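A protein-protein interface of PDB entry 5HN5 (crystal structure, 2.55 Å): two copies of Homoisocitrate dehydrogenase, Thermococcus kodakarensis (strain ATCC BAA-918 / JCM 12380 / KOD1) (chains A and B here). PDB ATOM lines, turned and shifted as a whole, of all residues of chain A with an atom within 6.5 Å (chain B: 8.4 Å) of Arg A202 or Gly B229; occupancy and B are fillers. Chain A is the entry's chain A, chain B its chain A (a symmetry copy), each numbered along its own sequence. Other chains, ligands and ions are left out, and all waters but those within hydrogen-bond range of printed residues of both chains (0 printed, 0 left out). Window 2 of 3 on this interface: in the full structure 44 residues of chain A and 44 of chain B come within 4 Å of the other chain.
Printed residues of chain A that touch a printed residue of chain B: Thr A197, Ile A198, Val A201 and Arg A202.
Hydrophobic or aromatic side chains of chain A within 4 Å of the printed part of chain B: Ile A198 and Val A201.
Of the 23 printed residues of chain B, 5 touch a printed residue of chain A.
Among the printed residues, no Asp or Glu carboxylate lies within 4 Å of a Lys or Arg side-chain nitrogen of the other chain.
Of the printed residues of chain B, Val A201 touches Leu B223 (3.6 Å) and Val B226 (3.7 Å).
Of the printed residues of chain A, Asp B222 touches Thr A197 (3.9 Å) and Ile A198 (3.1 Å).
The nearest residue of chain B that does not touch Arg A202 is Thr B225 (4.1 Å).
The nearest printed residue of chain A that does not touch Gly B229 is Ile A198 (7.3 Å).
The nearest printed residue of chain A that does not touch Leu B223 is Ile A198 (4.7 Å).
2 positions are printed for both chains.
Of the 8 pairs that touch across the chains among the printed residues, none has its exchanged pair printed and touching as well.
Among the printed residues, merely in contact across the chains: Ile A198 with Asp B222 (3.1 Å), Ile A198 with Thr B225 (3.4 Å), Val A201 with Leu B223 (3.6 Å), Arg A202 with Val B226 (3.6 Å), Val A201 with Val B226 (3.7 Å) and Thr A197 with Asp B222 (3.9 Å).
The backbone carbonyl oxygen of Val A201 sits close to a ring nitrogen (NE2) of His A227.
NH2 of Arg A202 is in hydrogen-bond range of O of Gly B229.
The side-chain hydroxyl of Thr A197 lies within hydrogen-bond range of the backbone NH of Leu B223 (3.5 Å).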
ATOM      1  N   THR A 197      -6.389 -28.109 -14.626  1.00  0.00           N
ATOM      2  CA  THR A 197      -7.564 -27.299 -14.303  1.00  0.00           C
ATOM      3  C   THR A 197      -7.250 -25.785 -14.446  1.00  0.00           C
ATOM      4  O   THR A 197      -8.109 -25.011 -14.844  1.00  0.00           O
ATOM      5  CB  THR A 197      -8.078 -27.542 -12.875  1.00  0.00           C
ATOM      6  OG1 THR A 197      -7.051 -27.218 -11.916  1.00  0.00           O
ATOM      7  CG2 THR A 197      -8.509 -28.979 -12.696  1.00  0.00           C
ATOM      8  N   ILE A 198      -6.019 -25.379 -14.111  1.00  0.00           N
ATOM      9  CA  ILE A 198      -5.590 -23.988 -14.228  1.00  0.00           C
ATOM     10  C   ILE A 198      -5.431 -23.596 -15.698  1.00  0.00           C
ATOM     11  O   ILE A 198      -5.929 -22.550 -16.120  1.00  0.00           O
ATOM     12  CB  ILE A 198      -4.253 -23.727 -13.480  1.00  0.00           C
ATOM     13  CG1 ILE A 198      -4.449 -23.810 -11.977  1.00  0.00           C
ATOM     14  CG2 ILE A 198      -3.687 -22.361 -13.829  1.00  0.00           C
ATOM     15  CD1 ILE A 198      -3.138 -24.034 -11.234  1.00  0.00           C
ATOM     16  N   LYS A 199      -4.723 -24.429 -16.464  1.00  0.00           N
ATOM     17  CA  LYS A 199      -4.571 -24.214 -17.895  1.00  0.00           C
ATOM     18  C   LYS A 199      -5.916 -24.172 -18.614  1.00  0.00           C
ATOM     19  O   LYS A 199      -6.050 -23.523 -19.666  1.00  0.00           O
ATOM     20  CB  LYS A 199      -3.707 -25.300 -18.536  1.00  0.00           C
ATOM     21  CG  LYS A 199      -2.233 -25.314 -18.155  1.00  0.00           C
ATOM     22  CD  LYS A 199      -1.530 -26.427 -18.915  1.00  0.00           C
ATOM     23  CE  LYS A 199      -0.054 -26.543 -18.566  1.00  0.00           C
ATOM     24  NZ  LYS A 199       0.156 -26.742 -17.110  1.00  0.00           N
ATOM     25  N   LEU A 200      -6.918 -24.861 -18.074  1.00  0.00           N
ATOM     26  CA  LEU A 200      -8.172 -24.986 -18.803  1.00  0.00           C
ATOM     27  C   LEU A 200      -9.014 -23.752 -18.615  1.00  0.00           C
ATOM     28  O   LEU A 200      -9.704 -23.338 -19.559  1.00  0.00           O
ATOM     29  CB  LEU A 200      -8.944 -26.253 -18.408  1.00  0.00           C
ATOM     30  CG  LEU A 200     -10.240 -26.530 -19.188  1.00  0.00           C
ATOM     31  CD1 LEU A 200     -10.017 -26.450 -20.692  1.00  0.00           C
ATOM     32  CD2 LEU A 200     -10.811 -27.886 -18.813  1.00  0.00           C
ATOM     33  N   VAL A 201      -8.967 -23.147 -17.425  1.00  0.00           N
ATOM     34  CA  VAL A 201      -9.667 -21.872 -17.246  1.00  0.00           C
ATOM     35  C   VAL A 201      -8.890 -20.683 -17.851  1.00  0.00           C
ATOM     36  O   VAL A 201      -9.521 -19.776 -18.353  1.00  0.00           O
ATOM     37  CB  VAL A 201     -10.253 -21.606 -15.819  1.00  0.00           C
ATOM     38  CG1 VAL A 201     -10.110 -22.777 -14.878  1.00  0.00           C
ATOM     39  CG2 VAL A 201      -9.753 -20.300 -15.218  1.00  0.00           C
ATOM     40  N   ARG A 202      -7.557 -20.709 -17.850  1.00  0.00           N
ATOM     41  CA  ARG A 202      -6.743 -19.559 -18.296  1.00  0.00           C
ATOM     42  C   ARG A 202      -6.381 -19.565 -19.780  1.00  0.00           C
ATOM     43  O   ARG A 202      -6.235 -18.512 -20.381  1.00  0.00           O
ATOM     44  CB  ARG A 202      -5.441 -19.480 -17.500  1.00  0.00           C
ATOM     45  CG  ARG A 202      -5.648 -19.267 -16.009  1.00  0.00           C
ATOM     46  CD  ARG A 202      -5.780 -17.800 -15.625  1.00  0.00           C
ATOM     47  NE  ARG A 202      -5.623 -17.614 -14.181  1.00  0.00           N
ATOM     48  CZ  ARG A 202      -4.479 -17.768 -13.508  1.00  0.00           C
ATOM     49  NH1 ARG A 202      -3.351 -18.109 -14.134  1.00  0.00           N
ATOM     50  NH2 ARG A 202      -4.463 -17.585 -12.192  1.00  0.00           N
ATOM     51  N   ASN A 203      -6.208 -20.745 -20.360  1.00  0.00           N
ATOM     52  CA  ASN A 203      -5.851 -20.876 -21.758  1.00  0.00           C
ATOM     53  C   ASN A 203      -6.713 -21.947 -22.397  1.00  0.00           C
ATOM     54  O   ASN A 203      -6.192 -22.927 -22.933  1.00  0.00           O
ATOM     55  CB  ASN A 203      -4.373 -21.239 -21.882  1.00  0.00           C
ATOM     56  CG  ASN A 203      -3.865 -21.176 -23.313  1.00  0.00           C
ATOM     57  OD1 ASN A 203      -4.452 -20.508 -24.178  1.00  0.00           O
ATOM     58  ND2 ASN A 203      -2.766 -21.869 -23.574  1.00  0.00           N
ATOM     59  N   PRO A 204      -8.044 -21.751 -22.382  1.00  0.00           N
ATOM     60  CA  PRO A 204      -8.973 -22.803 -22.835  1.00  0.00           C
ATOM     61  C   PRO A 204      -8.735 -23.368 -24.229  1.00  0.00           C
ATOM     62  O   PRO A 204      -8.924 -24.566 -24.450  1.00  0.00           O
ATOM     63  CB  PRO A 204     -10.322 -22.115 -22.807  1.00  0.00           C
ATOM     64  CG  PRO A 204     -10.021 -20.651 -22.878  1.00  0.00           C
ATOM     65  CD  PRO A 204      -8.754 -20.495 -22.084  1.00  0.00           C
ATOM     66  N   TRP A 205      -8.322 -22.528 -25.162  1.00  0.00           N
ATOM     67  CA  TRP A 205      -8.514 -22.854 -26.574  1.00  0.00           C
ATOM     68  C   TRP A 205      -7.334 -23.519 -27.189  1.00  0.00           C
ATOM     69  O   TRP A 205      -7.370 -23.780 -28.369  1.00  0.00           O
ATOM     70  CB  TRP A 205      -8.849 -21.607 -27.375  1.00  0.00           C
ATOM     71  CG  TRP A 205      -9.902 -20.787 -26.748  1.00  0.00           C
ATOM     72  CD1 TRP A 205      -9.774 -19.519 -26.248  1.00  0.00           C
ATOM     73  CD2 TRP A 205     -11.257 -21.173 -26.525  1.00  0.00           C
ATOM     74  NE1 TRP A 205     -10.985 -19.085 -25.741  1.00  0.00           N
ATOM     75  CE2 TRP A 205     -11.909 -20.084 -25.898  1.00  0.00           C
ATOM     76  CE3 TRP A 205     -11.993 -22.326 -26.815  1.00  0.00           C
ATOM     77  CZ2 TRP A 205     -13.249 -20.123 -25.548  1.00  0.00           C
ATOM     78  CZ3 TRP A 205     -13.325 -22.368 -26.464  1.00  0.00           C
ATOM     79  CH2 TRP A 205     -13.942 -21.282 -25.838  1.00  0.00           C
ATOM     80  N   HIS A 227     -16.373 -21.477 -20.104  1.00  0.00           N
ATOM     81  CA  HIS A 227     -16.051 -20.761 -21.328  1.00  0.00           C
ATOM     82  C   HIS A 227     -17.147 -20.726 -22.376  1.00  0.00           C
ATOM     83  O   HIS A 227     -16.910 -20.219 -23.468  1.00  0.00           O
ATOM     84  CB  HIS A 227     -14.847 -21.379 -21.985  1.00  0.00           C
ATOM     85  CG  HIS A 227     -13.638 -21.360 -21.124  1.00  0.00           C
ATOM     86  ND1 HIS A 227     -13.243 -20.241 -20.429  1.00  0.00           N
ATOM     87  CD2 HIS A 227     -12.744 -22.326 -20.827  1.00  0.00           C
ATOM     88  CE1 HIS A 227     -12.145 -20.512 -19.755  1.00  0.00           C
ATOM     89  NE2 HIS A 227     -11.822 -21.773 -19.978  1.00  0.00           N
ATOM     90  N   ILE B  98      -6.631 -20.338  -0.107  1.00  0.00           N
ATOM     91  CA  ILE B  98      -6.403 -19.456  -1.260  1.00  0.00           C
ATOM     92  C   ILE B  98      -6.960 -18.060  -0.948  1.00  0.00           C
ATOM     93  O   ILE B  98      -8.170 -17.912  -0.748  1.00  0.00           O
ATOM     94  CB  ILE B  98      -7.057 -19.967  -2.565  1.00  0.00           C
ATOM     95  CG1 ILE B  98      -6.413 -21.275  -3.064  1.00  0.00           C
ATOM     96  CG2 ILE B  98      -6.882 -18.921  -3.659  1.00  0.00           C
ATOM     97  CD1 ILE B  98      -6.823 -22.530  -2.332  1.00  0.00           C
ATOM     98  N   PRO B  99      -6.086 -17.032  -0.899  1.00  0.00           N
ATOM     99  CA  PRO B  99      -6.543 -15.685  -0.541  1.00  0.00           C
ATOM    100  C   PRO B  99      -6.686 -14.736  -1.725  1.00  0.00           C
ATOM    101  O   PRO B  99      -5.849 -14.744  -2.631  1.00  0.00           O
ATOM    102  CB  PRO B  99      -5.415 -15.193   0.361  1.00  0.00           C
ATOM    103  CG  PRO B  99      -4.192 -15.855  -0.186  1.00  0.00           C
ATOM    104  CD  PRO B  99      -4.614 -17.073  -0.972  1.00  0.00           C
ATOM    105  N   ASP B 100      -7.754 -13.939  -1.719  1.00  0.00           N
ATOM    106  CA  ASP B 100      -7.846 -12.745  -2.578  1.00  0.00           C
ATOM    107  C   ASP B 100      -7.176 -11.669  -1.759  1.00  0.00           C
ATOM    108  O   ASP B 100      -7.706 -11.242  -0.731  1.00  0.00           O
ATOM    109  CB  ASP B 100      -9.303 -12.370  -2.868  1.00  0.00           C
ATOM    110  CG  ASP B 100      -9.441 -11.218  -3.863  1.00  0.00           C
ATOM    111  OD1 ASP B 100      -8.631 -11.111  -4.809  1.00  0.00           O
ATOM    112  OD2 ASP B 100     -10.396 -10.429  -3.710  1.00  0.00           O
ATOM    113  N   LEU B 101      -5.994 -11.259  -2.182  1.00  0.00           N
ATOM    114  CA  LEU B 101      -5.059 -10.663  -1.236  1.00  0.00           C
ATOM    115  C   LEU B 101      -5.384  -9.195  -0.939  1.00  0.00           C
ATOM    116  O   LEU B 101      -4.941  -8.634   0.073  1.00  0.00           O
ATOM    117  CB  LEU B 101      -3.617 -10.861  -1.724  1.00  0.00           C
ATOM    118  CG  LEU B 101      -2.547 -11.217  -0.674  1.00  0.00           C
ATOM    119  CD1 LEU B 101      -3.063 -11.962   0.562  1.00  0.00           C
ATOM    120  CD2 LEU B 101      -1.429 -12.012  -1.342  1.00  0.00           C
ATOM    121  N   TRP B 205     -16.333 -17.620  -3.247  1.00  0.00           N
ATOM    122  CA  TRP B 205     -16.149 -17.199  -1.859  1.00  0.00           C
ATOM    123  C   TRP B 205     -17.231 -17.670  -0.953  1.00  0.00           C
ATOM    124  O   TRP B 205     -17.203 -17.328   0.206  1.00  0.00           O
ATOM    125  CB  TRP B 205     -16.053 -15.685  -1.763  1.00  0.00           C
ATOM    126  CG  TRP B 205     -15.121 -15.105  -2.748  1.00  0.00           C
ATOM    127  CD1 TRP B 205     -15.432 -14.268  -3.786  1.00  0.00           C
ATOM    128  CD2 TRP B 205     -13.713 -15.327  -2.816  1.00  0.00           C
ATOM    129  NE1 TRP B 205     -14.287 -13.940  -4.488  1.00  0.00           N
ATOM    130  CE2 TRP B 205     -13.221 -14.579  -3.912  1.00  0.00           C
ATOM    131  CE3 TRP B 205     -12.814 -16.067  -2.042  1.00  0.00           C
ATOM    132  CZ2 TRP B 205     -11.878 -14.564  -4.256  1.00  0.00           C
ATOM    133  CZ3 TRP B 205     -11.480 -16.055  -2.385  1.00  0.00           C
ATOM    134  CH2 TRP B 205     -11.020 -15.315  -3.478  1.00  0.00           C
ATOM    135  N   ASP B 222      -5.820 -26.836  -6.735  1.00  0.00           N
ATOM    136  CA  ASP B 222      -5.174 -26.192  -7.884  1.00  0.00           C
ATOM    137  C   ASP B 222      -6.131 -25.278  -8.670  1.00  0.00           C
ATOM    138  O   ASP B 222      -5.728 -24.213  -9.148  1.00  0.00           O
ATOM    139  CB  ASP B 222      -4.607 -27.238  -8.832  1.00  0.00           C
ATOM    140  CG  ASP B 222      -3.140 -27.470  -8.637  1.00  0.00           C
ATOM    141  OD1 ASP B 222      -2.669 -27.461  -7.487  1.00  0.00           O
ATOM    142  OD2 ASP B 222      -2.450 -27.672  -9.657  1.00  0.00           O
ATOM    143  N   LEU B 223      -7.381 -25.703  -8.829  1.00  0.00           N
ATOM    144  CA  LEU B 223      -8.385 -24.882  -9.502  1.00  0.00           C
ATOM    145  C   LEU B 223      -8.675 -23.591  -8.747  1.00  0.00           C
ATOM    146  O   LEU B 223      -8.805 -22.545  -9.364  1.00  0.00           O
ATOM    147  CB  LEU B 223      -9.708 -25.654  -9.688  1.00  0.00           C
ATOM    148  CG  LEU B 223     -10.854 -24.891 -10.375  1.00  0.00           C
ATOM    149  CD1 LEU B 223     -10.483 -24.497 -11.790  1.00  0.00           C
ATOM    150  CD2 LEU B 223     -12.128 -25.699 -10.409  1.00  0.00           C
ATOM    151  N   ALA B 224      -8.828 -23.683  -7.425  1.00  0.00           N
ATOM    152  CA  ALA B 224      -9.145 -22.523  -6.580  1.00  0.00           C
ATOM    153  C   ALA B 224      -8.130 -21.399  -6.769  1.00  0.00           C
ATOM    154  O   ALA B 224      -8.433 -20.223  -6.716  1.00  0.00           O
ATOM    155  CB  ALA B 224      -9.165 -22.945  -5.130  1.00  0.00           C
ATOM    156  N   THR B 225      -6.909 -21.817  -6.994  1.00  0.00           N
ATOM    157  CA  THR B 225      -5.801 -20.969  -7.356  1.00  0.00           C
ATOM    158  C   THR B 225      -6.012 -19.870  -8.389  1.00  0.00           C
ATOM    159  O   THR B 225      -5.324 -18.851  -8.343  1.00  0.00           O
ATOM    160  CB  THR B 225      -4.666 -21.900  -7.809  1.00  0.00           C
ATOM    161  OG1 THR B 225      -3.752 -22.015  -6.712  1.00  0.00           O
ATOM    162  CG2 THR B 225      -3.972 -21.454  -9.118  1.00  0.00           C
ATOM    163  N   VAL B 226      -6.922 -20.063  -9.334  1.00  0.00           N
ATOM    164  CA  VAL B 226      -7.176 -19.005 -10.313  1.00  0.00           C
ATOM    165  C   VAL B 226      -7.660 -17.712  -9.660  1.00  0.00           C
ATOM    166  O   VAL B 226      -7.390 -16.644 -10.194  1.00  0.00           O
ATOM    167  CB  VAL B 226      -8.174 -19.418 -11.412  1.00  0.00           C
ATOM    168  CG1 VAL B 226      -7.612 -20.609 -12.168  1.00  0.00           C
ATOM    169  CG2 VAL B 226      -9.574 -19.674 -10.838  1.00  0.00           C
ATOM    170  N   HIS B 227      -8.355 -17.824  -8.521  1.00  0.00           N
ATOM    171  CA  HIS B 227      -8.839 -16.674  -7.773  1.00  0.00           C
ATOM    172  C   HIS B 227      -7.807 -15.968  -6.916  1.00  0.00           C
ATOM    173  O   HIS B 227      -8.168 -15.047  -6.188  1.00  0.00           O
ATOM    174  CB  HIS B 227      -9.953 -17.089  -6.853  1.00  0.00           C
ATOM    175  CG  HIS B 227     -11.113 -17.678  -7.568  1.00  0.00           C
ATOM    176  ND1 HIS B 227     -11.655 -17.105  -8.695  1.00  0.00           N
ATOM    177  CD2 HIS B 227     -11.826 -18.798  -7.332  1.00  0.00           C
ATOM    178  CE1 HIS B 227     -12.666 -17.838  -9.113  1.00  0.00           C
ATOM    179  NE2 HIS B 227     -12.790 -18.873  -8.303  1.00  0.00           N
ATOM    180  N   ALA B 228      -6.556 -16.419  -6.933  1.00  0.00           N
ATOM    181  CA  ALA B 228      -5.484 -15.687  -6.262  1.00  0.00           C
ATOM    182  C   ALA B 228      -4.522 -15.103  -7.279  1.00  0.00           C
ATOM    183  O   ALA B 228      -3.587 -14.404  -6.911  1.00  0.00           O
ATOM    184  CB  ALA B 228      -4.746 -16.572  -5.277  1.00  0.00           C
ATOM    185  N   GLY B 229      -4.747 -15.384  -8.555  1.00  0.00           N
ATOM    186  CA  GLY B 229      -3.963 -14.764  -9.610  1.00  0.00           C
ATOM    187  C   GLY B 229      -2.761 -15.589  -9.994  1.00  0.00           C
ATOM    188  O   GLY B 229      -2.456 -15.715 -11.176  1.00  0.00           O
ATOM    189  N   SER B 230      -2.067 -16.119  -8.992  1.00  0.00           N
ATOM    190  CA  SER B 230      -1.023 -17.108  -9.199  1.00  0.00           C
ATOM    191  C   SER B 230      -1.104 -18.181  -8.130  1.00  0.00           C
ATOM    192  O   SER B 230      -1.513 -17.938  -6.989  1.00  0.00           O
ATOM    193  CB  SER B 230       0.361 -16.488  -9.164  1.00  0.00           C
ATOM    194  OG  SER B 230       1.343 -17.477  -9.412  1.00  0.00           O
ATOM    195  N   ILE B 231      -0.727 -19.384  -8.533  1.00  0.00           N
ATOM    196  CA  ILE B 231      -0.648 -20.514  -7.638  1.00  0.00           C
ATOM    197  C   ILE B 231       0.432 -20.202  -6.570  1.00  0.00           C
ATOM    198  O   ILE B 231       0.316 -20.602  -5.407  1.00  0.00           O
ATOM    199  CB  ILE B 231      -0.355 -21.816  -8.438  1.00  0.00           C
ATOM    200  CG1 ILE B 231      -0.536 -23.052  -7.551  1.00  0.00           C
ATOM    201  CG2 ILE B 231       1.039 -21.792  -9.069  1.00  0.00           C
ATOM    202  CD1 ILE B 231      -0.135 -24.370  -8.196  1.00  0.00           C
ATOM    203  N   GLY B 232       1.448 -19.451  -6.985  1.00  0.00           N
ATOM    204  CA  GLY B 232       2.570 -19.101  -6.145  1.00  0.00           C
ATOM    205  C   GLY B 232       2.355 -18.123  -4.998  1.00  0.00           C
ATOM    206  O   GLY B 232       3.327 -17.690  -4.418  1.00  0.00           O
ATOM    207  N   ILE B 233       1.118 -17.768  -4.659  1.00  0.00           N
ATOM    208  CA  ILE B 233       0.870 -17.055  -3.410  1.00  0.00           C
ATOM    209  C   ILE B 233       0.171 -17.959  -2.389  1.00  0.00           C
ATOM    210  O   ILE B 233      -0.102 -17.527  -1.253  1.00  0.00           O
ATOM    211  CB  ILE B 233       0.081 -15.713  -3.588  1.00  0.00           C
ATOM    212  CG1 ILE B 233      -1.404 -15.933  -3.828  1.00  0.00           C
ATOM    213  CG2 ILE B 233       0.662 -14.847  -4.703  1.00  0.00           C
ATOM    214  CD1 ILE B 233      -2.179 -14.633  -3.811  1.00  0.00           C
ATOM    215  N   VAL B 234      -0.102 -19.210  -2.765  1.00  0.00           N
ATOM    216  CA  VAL B 234      -0.953 -20.054  -1.936  1.00  0.00           C
ATOM    217  C   VAL B 234      -0.124 -20.937  -0.983  1.00  0.00           C
ATOM    218  O   VAL B 234       0.795 -21.634  -1.425  1.00  0.00           O
ATOM    219  CB  VAL B 234      -1.891 -20.897  -2.810  1.00  0.00           C
ATOM    220  CG1 VAL B 234      -2.810 -21.761  -1.949  1.00  0.00           C
ATOM    221  CG2 VAL B 234      -2.721 -19.987  -3.708  1.00  0.00           C
ATOM    222  N   ASN B 263       7.914 -16.369  -7.039  1.00  0.00           N
ATOM    223  CA  ASN B 263       7.091 -15.768  -6.014  1.00  0.00           C
ATOM    224  C   ASN B 263       7.315 -16.490  -4.676  1.00  0.00           C
ATOM    225  O   ASN B 263       7.010 -17.673  -4.574  1.00  0.00           O
ATOM    226  CB  ASN B 263       5.623 -15.865  -6.435  1.00  0.00           C
ATOM    227  CG  ASN B 263       4.706 -15.056  -5.554  1.00  0.00           C
ATOM    228  OD1 ASN B 263       5.109 -14.569  -4.498  1.00  0.00           O
ATOM    229  ND2 ASN B 263       3.458 -14.910  -5.976  1.00  0.00           N
ATOM    230  N   PRO B 300       6.559 -11.618 -11.674  1.00  0.00           N
ATOM    231  CA  PRO B 300       6.037 -11.784 -13.047  1.00  0.00           C
ATOM    232  C   PRO B 300       4.814 -12.668 -13.186  1.00  0.00           C
ATOM    233  O   PRO B 300       3.985 -12.415 -14.059  1.00  0.00           O
ATOM    234  CB  PRO B 300       7.210 -12.413 -13.796  1.00  0.00           C
ATOM    235  CG  PRO B 300       8.410 -11.861 -13.107  1.00  0.00           C
ATOM    236  CD  PRO B 300       8.033 -11.741 -11.653  1.00  0.00           C
ATOM    237  N   ASP B 301       4.697 -13.693 -12.345  1.00  0.00           N
ATOM    238  CA  ASP B 301       3.537 -14.575 -12.398  1.00  0.00           C
ATOM    239  C   ASP B 301       2.282 -13.858 -11.949  1.00  0.00           C
ATOM    240  O   ASP B 301       1.176 -14.308 -12.245  1.00  0.00           O
ATOM    241  CB  ASP B 301       3.749 -15.820 -11.543  1.00  0.00           C
ATOM    242  CG  ASP B 301       4.116 -15.489 -10.107  1.00  0.00           C
ATOM    243  OD1 ASP B 301       5.282 -15.084  -9.908  1.00  0.00           O
ATOM    244  OD2 ASP B 301       3.244 -15.634  -9.207  1.00  0.00           O
ATOM    245  N   MET B 302       2.457 -12.758 -11.218  1.00  0.00           N
ATOM    246  CA  MET B 302       1.354 -11.890 -10.830  1.00  0.00           C
ATOM    247  C   MET B 302       1.227 -10.686 -11.782  1.00  0.00           C
ATOM    248  O   MET B 302       0.324  -9.869 -11.620  1.00  0.00           O
ATOM    249  CB  MET B 302       1.540 -11.401  -9.384  1.00  0.00           C
ATOM    250  CG  MET B 302       1.519 -12.493  -8.314  1.00  0.00           C
ATOM    251  SD  MET B 302      -0.102 -13.263  -8.085  1.00  0.00           S
ATOM    252  CE  MET B 302      -1.031 -12.012  -7.197  1.00  0.00           C
ATOM    253  N   GLY B 303       2.120 -10.588 -12.772  1.00  0.00           N
ATOM    254  CA  GLY B 303       2.106  -9.501 -13.761  1.00  0.00           C
ATOM    255  C   GLY B 303       3.097  -8.367 -13.518  1.00  0.00           C
ATOM    256  O   GLY B 303       3.261  -7.507 -14.377  1.00  0.00           O
